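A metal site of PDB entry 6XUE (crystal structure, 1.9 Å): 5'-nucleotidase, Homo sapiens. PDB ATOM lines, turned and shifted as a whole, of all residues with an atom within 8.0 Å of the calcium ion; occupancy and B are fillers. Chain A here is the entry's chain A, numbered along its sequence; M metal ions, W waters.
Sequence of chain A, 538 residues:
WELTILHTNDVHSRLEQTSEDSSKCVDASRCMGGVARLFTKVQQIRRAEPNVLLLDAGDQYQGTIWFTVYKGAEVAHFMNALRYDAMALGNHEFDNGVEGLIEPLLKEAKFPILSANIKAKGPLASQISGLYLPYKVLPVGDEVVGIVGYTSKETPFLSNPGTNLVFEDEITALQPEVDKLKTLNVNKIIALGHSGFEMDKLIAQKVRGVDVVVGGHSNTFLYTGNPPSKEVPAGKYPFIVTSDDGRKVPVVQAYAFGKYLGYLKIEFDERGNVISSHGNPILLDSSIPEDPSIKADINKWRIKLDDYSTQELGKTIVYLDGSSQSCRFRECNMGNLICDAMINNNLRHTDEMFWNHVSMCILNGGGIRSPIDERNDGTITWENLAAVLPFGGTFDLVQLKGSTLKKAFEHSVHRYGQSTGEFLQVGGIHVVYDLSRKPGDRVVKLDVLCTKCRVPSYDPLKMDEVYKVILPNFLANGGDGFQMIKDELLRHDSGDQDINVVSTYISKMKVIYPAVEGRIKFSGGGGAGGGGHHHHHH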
ATOM      1  N   LYS A 182      20.763 -26.444  19.657  1.00  0.00           N
ATOM      2  CA  LYS A 182      20.858 -25.262  18.758  1.00  0.00           C
ATOM      3  C   LYS A 182      20.608 -23.948  19.524  1.00  0.00           C
ATOM      4  O   LYS A 182      21.333 -22.980  19.326  1.00  0.00           O
ATOM      5  CB  LYS A 182      19.848 -25.377  17.588  1.00  0.00           C
ATOM      6  CG  LYS A 182      20.092 -26.542  16.642  1.00  0.00           C
ATOM      7  CD  LYS A 182      21.143 -26.197  15.603  1.00  0.00           C
ATOM      8  CE  LYS A 182      21.869 -27.428  15.154  1.00  0.00           C
ATOM      9  NZ  LYS A 182      23.334 -27.215  15.181  1.00  0.00           N
ATOM     10  N   VAL A 186      25.056 -24.650  20.238  1.00  0.00           N
ATOM     11  CA  VAL A 186      25.866 -25.837  19.937  1.00  0.00           C
ATOM     12  C   VAL A 186      25.566 -26.140  18.462  1.00  0.00           C
ATOM     13  O   VAL A 186      24.475 -26.629  18.138  1.00  0.00           O
ATOM     14  CB  VAL A 186      25.608 -27.035  20.887  1.00  0.00           C
ATOM     15  CG1 VAL A 186      26.469 -28.237  20.497  1.00  0.00           C
ATOM     16  CG2 VAL A 186      25.859 -26.648  22.344  1.00  0.00           C
ATOM     17  N   ASN A 187      26.529 -25.788  17.573  1.00  0.00           N
ATOM     18  CA  ASN A 187      26.417 -25.902  16.114  1.00  0.00           C
ATOM     19  C   ASN A 187      26.979 -27.201  15.514  1.00  0.00           C
ATOM     20  O   ASN A 187      26.773 -27.454  14.323  1.00  0.00           O
ATOM     21  CB  ASN A 187      27.016 -24.662  15.429  1.00  0.00           C
ATOM     22  CG  ASN A 187      28.492 -24.384  15.693  1.00  0.00           C
ATOM     23  OD1 ASN A 187      29.314 -25.290  15.885  1.00  0.00           O
ATOM     24  ND2 ASN A 187      28.869 -23.121  15.682  1.00  0.00           N
ATOM     25  N   LYS A 188      27.694 -28.019  16.322  1.00  0.00           N
ATOM     26  CA  LYS A 188      28.264 -29.310  15.918  1.00  0.00           C
ATOM     27  C   LYS A 188      27.606 -30.416  16.769  1.00  0.00           C
ATOM     28  O   LYS A 188      27.720 -30.385  18.002  1.00  0.00           O
ATOM     29  CB  LYS A 188      29.809 -29.319  16.018  1.00  0.00           C
ATOM     30  CG  LYS A 188      30.488 -28.377  15.010  1.00  0.00           C
ATOM     31  CD  LYS A 188      31.999 -28.222  15.227  1.00  0.00           C
ATOM     32  CE  LYS A 188      32.387 -27.274  16.361  1.00  0.00           C
ATOM     33  NZ  LYS A 188      32.037 -25.851  16.062  1.00  0.00           N
ATOM     34  N   ILE A 189      26.848 -31.331  16.106  1.00  0.00           N
ATOM     35  CA  ILE A 189      26.068 -32.369  16.796  1.00  0.00           C
ATOM     36  C   ILE A 189      26.333 -33.799  16.252  1.00  0.00           C
ATOM     37  O   ILE A 189      26.142 -34.077  15.057  1.00  0.00           O
ATOM     38  CB  ILE A 189      24.553 -32.015  16.818  1.00  0.00           C
ATOM     39  CG1 ILE A 189      24.300 -30.789  17.742  1.00  0.00           C
ATOM     40  CG2 ILE A 189      23.644 -33.225  17.259  1.00  0.00           C
ATOM     41  CD1 ILE A 189      23.151 -30.018  17.434  1.00  0.00           C
ATOM     42  N   ILE A 190      26.738 -34.698  17.173  1.00  0.00           N
ATOM     43  CA  ILE A 190      26.941 -36.127  16.891  1.00  0.00           C
ATOM     44  C   ILE A 190      25.821 -36.933  17.545  1.00  0.00           C
ATOM     45  O   ILE A 190      25.565 -36.788  18.741  1.00  0.00           O
ATOM     46  CB  ILE A 190      28.329 -36.657  17.384  1.00  0.00           C
ATOM     47  CG1 ILE A 190      29.507 -35.762  16.917  1.00  0.00           C
ATOM     48  CG2 ILE A 190      28.543 -38.146  16.984  1.00  0.00           C
ATOM     49  CD1 ILE A 190      30.848 -36.157  17.535  1.00  0.00           C
ATOM     50  N   GLY A 209      19.443 -31.122  11.927  1.00  0.00           N
ATOM     51  CA  GLY A 209      20.571 -30.610  12.694  1.00  0.00           C
ATOM     52  C   GLY A 209      21.700 -31.580  13.017  1.00  0.00           C
ATOM     53  O   GLY A 209      22.804 -31.139  13.342  1.00  0.00           O
ATOM     54  N   VAL A 210      21.441 -32.912  12.936  1.00  0.00           N
ATOM     55  CA  VAL A 210      22.482 -33.937  13.190  1.00  0.00           C
ATOM     56  C   VAL A 210      23.576 -33.835  12.108  1.00  0.00           C
ATOM     57  O   VAL A 210      23.243 -33.765  10.923  1.00  0.00           O
ATOM     58  CB  VAL A 210      21.902 -35.387  13.344  1.00  0.00           C
ATOM     59  CG1 VAL A 210      23.005 -36.432  13.387  1.00  0.00           C
ATOM     60  CG2 VAL A 210      21.027 -35.494  14.584  1.00  0.00           C
ATOM     61  N   ASP A 211      24.857 -33.746  12.508  1.00  0.00           N
ATOM     62  CA  ASP A 211      25.964 -33.637  11.549  1.00  0.00           C
ATOM     63  C   ASP A 211      26.600 -34.977  11.178  1.00  0.00           C
ATOM     64  O   ASP A 211      27.068 -35.120  10.042  1.00  0.00           O
ATOM     65  CB  ASP A 211      27.044 -32.665  12.027  1.00  0.00           C
ATOM     66  CG  ASP A 211      26.540 -31.249  12.242  1.00  0.00           C
ATOM     67  OD1 ASP A 211      26.050 -30.632  11.258  1.00  0.00           O
ATOM     68  OD2 ASP A 211      26.626 -30.755  13.385  1.00  0.00           O
ATOM     69  N   VAL A 212      26.680 -35.921  12.151  1.00  0.00           N
ATOM     70  CA  VAL A 212      27.303 -37.253  12.021  1.00  0.00           C
ATOM     71  C   VAL A 212      26.493 -38.264  12.873  1.00  0.00           C
ATOM     72  O   VAL A 212      26.078 -37.931  13.977  1.00  0.00           O
ATOM     73  CB  VAL A 212      28.778 -37.250  12.531  1.00  0.00           C
ATOM     74  CG1 VAL A 212      29.489 -38.573  12.221  1.00  0.00           C
ATOM     75  CG2 VAL A 212      29.590 -36.073  11.977  1.00  0.00           C
ATOM     76  N   ARG A 247      21.204 -31.738   3.486  1.00  0.00           N
ATOM     77  CA  ARG A 247      22.638 -31.840   3.806  1.00  0.00           C
ATOM     78  C   ARG A 247      23.169 -33.274   3.583  1.00  0.00           C
ATOM     79  O   ARG A 247      22.385 -34.218   3.423  1.00  0.00           O
ATOM     80  CB  ARG A 247      22.912 -31.384   5.251  1.00  0.00           C
ATOM     81  CG  ARG A 247      22.538 -29.931   5.555  1.00  0.00           C
ATOM     82  CD  ARG A 247      22.515 -29.594   7.048  1.00  0.00           C
ATOM     83  NE  ARG A 247      21.749 -30.574   7.820  1.00  0.00           N
ATOM     84  CZ  ARG A 247      22.270 -31.393   8.722  1.00  0.00           C
ATOM     85  NH1 ARG A 247      21.499 -32.291   9.326  1.00  0.00           N
ATOM     86  NH2 ARG A 247      23.562 -31.325   9.029  1.00  0.00           N
ATOM     87  N   PHE A 268      34.950 -29.072   9.412  1.00  0.00           N
ATOM     88  CA  PHE A 268      33.767 -28.253   9.682  1.00  0.00           C
ATOM     89  C   PHE A 268      34.056 -26.798   9.266  1.00  0.00           C
ATOM     90  O   PHE A 268      35.195 -26.343   9.358  1.00  0.00           O
ATOM     91  CB  PHE A 268      33.425 -28.255  11.184  1.00  0.00           C
ATOM     92  CG  PHE A 268      32.716 -29.477  11.731  1.00  0.00           C
ATOM     93  CD1 PHE A 268      31.337 -29.617  11.594  1.00  0.00           C
ATOM     94  CD2 PHE A 268      33.418 -30.454  12.424  1.00  0.00           C
ATOM     95  CE1 PHE A 268      30.685 -30.736  12.112  1.00  0.00           C
ATOM     96  CE2 PHE A 268      32.767 -31.573  12.942  1.00  0.00           C
ATOM     97  CZ  PHE A 268      31.395 -31.703  12.793  1.00  0.00           C
ATOM     98  N   ASP A 269      32.997 -26.056   8.880  1.00  0.00           N
ATOM     99  CA  ASP A 269      33.141 -24.621   8.633  1.00  0.00           C
ATOM    100  C   ASP A 269      32.886 -23.914   9.991  1.00  0.00           C
ATOM    101  O   ASP A 269      32.599 -24.594  10.987  1.00  0.00           O
ATOM    102  CB  ASP A 269      32.212 -24.106   7.505  1.00  0.00           C
ATOM    103  CG  ASP A 269      30.700 -24.112   7.756  1.00  0.00           C
ATOM    104  OD1 ASP A 269      30.291 -24.273   8.925  1.00  0.00           O
ATOM    105  OD2 ASP A 269      29.937 -23.936   6.782  1.00  0.00           O
ATOM    106  N   ARG A 271      30.373 -22.263  11.047  1.00  0.00           N
ATOM    107  CA  ARG A 271      28.983 -22.386  11.501  1.00  0.00           C
ATOM    108  C   ARG A 271      28.604 -23.824  11.874  1.00  0.00           C
ATOM    109  O   ARG A 271      27.443 -24.102  12.200  1.00  0.00           O
ATOM    110  CB  ARG A 271      28.011 -21.774  10.461  1.00  0.00           C
ATOM    111  CG  ARG A 271      28.288 -20.298  10.139  1.00  0.00           C
ATOM    112  CD  ARG A 271      27.154 -19.660   9.361  1.00  0.00           C
ATOM    113  NE  ARG A 271      25.982 -19.440  10.205  1.00  0.00           N
ATOM    114  CZ  ARG A 271      24.865 -18.827   9.817  1.00  0.00           C
ATOM    115  NH1 ARG A 271      24.748 -18.353   8.579  1.00  0.00           N
ATOM    116  NH2 ARG A 271      23.852 -18.684  10.662  1.00  0.00           N
ATOM    117  N   GLY A 272      29.596 -24.717  11.883  1.00  0.00           N
ATOM    118  CA  GLY A 272      29.402 -26.123  12.256  1.00  0.00           C
ATOM    119  C   GLY A 272      28.855 -27.035  11.178  1.00  0.00           C
ATOM    120  O   GLY A 272      28.362 -28.114  11.503  1.00  0.00           O
ATOM    121  N   ASN A 273      28.949 -26.625   9.884  1.00  0.00           N
ATOM    122  CA  ASN A 273      28.498 -27.455   8.751  1.00  0.00           C
ATOM    123  C   ASN A 273      29.647 -28.311   8.254  1.00  0.00           C
ATOM    124  O   ASN A 273      30.772 -27.804   8.114  1.00  0.00           O
ATOM    125  CB  ASN A 273      27.997 -26.580   7.590  1.00  0.00           C
ATOM    126  CG  ASN A 273      26.891 -25.620   7.950  1.00  0.00           C
ATOM    127  OD1 ASN A 273      27.001 -24.416   7.748  1.00  0.00           O
ATOM    128  ND2 ASN A 273      25.792 -26.133   8.469  1.00  0.00           N
ATOM    129  N   VAL A 274      29.376 -29.615   7.955  1.00  0.00           N
ATOM    130  CA  VAL A 274      30.383 -30.535   7.425  1.00  0.00           C
ATOM    131  C   VAL A 274      30.759 -30.138   5.990  1.00  0.00           C
ATOM    132  O   VAL A 274      29.895 -30.082   5.119  1.00  0.00           O
ATOM    133  CB  VAL A 274      30.006 -32.048   7.528  1.00  0.00           C
ATOM    134  CG1 VAL A 274      31.128 -32.934   6.999  1.00  0.00           C
ATOM    135  CG2 VAL A 274      29.645 -32.442   8.968  1.00  0.00           C
HETATM  136 CA    CA M   1      25.972 -28.500  12.430  1.00  0.00          CA
HETATM  137  O   HOH W   1      23.594 -28.647  12.780  1.00  0.00           O
HETATM  138  O   HOH W   2      25.431 -25.991  11.991  1.00  0.00           O
HETATM  139  O   HOH W   3      24.556 -28.359   9.616  1.00  0.00           O
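The side-chain amide oxygen (OD1) of Asn 187 lies within hydrogen-bond range of the side-chain amino group (NZ) of Lys 188. The backbone NH (N) of Asp 211 is in hydrogen-bond range of the backbone carbonyl oxygen (O) of Ile 189 (2.9 Å). The guanidinium group (NH2) of Arg 247 sits close to the side-chain carboxylate (OD1) of Asp 211 (3.4 Å). The backbone NH (N) of Gly 272 lies within hydrogen-bond range of the side-chain carboxylate (OD1) of Asp 269 (3.1 Å).
Three residues have an atom within 4 Å of the calcium ion: Asn 187, Asp 211 and Gly 272. Along chain A the residues within 4 Å of the calcium ion span positions 187 to 272.
The calcium ion is bound by O of Asn 187, 2.3 Å away. Water W1 is bound to the calcium ion (2.4 Å). The calcium ion is bound by the side-chain carboxylate (OD1) of Asp 211. The calcium ion is bound by OD2 of Asp 211 (2.5 Å). O of Gly 272 binds the calcium ion. The calcium ion is bound by water W2 (2.6 Å). The calcium ion has six donor atoms within binding distance.
Water W1 bridges the backbone carbonyl oxygen of Gly 209 (2.7 Å) and the side-chain amino group of Lys 182 (2.8 Å). Water W3 lies within hydrogen-bond range of the side-chain amide nitrogen (ND2) of Asn 273 and the guanidinium group (NH2) of Arg 247.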
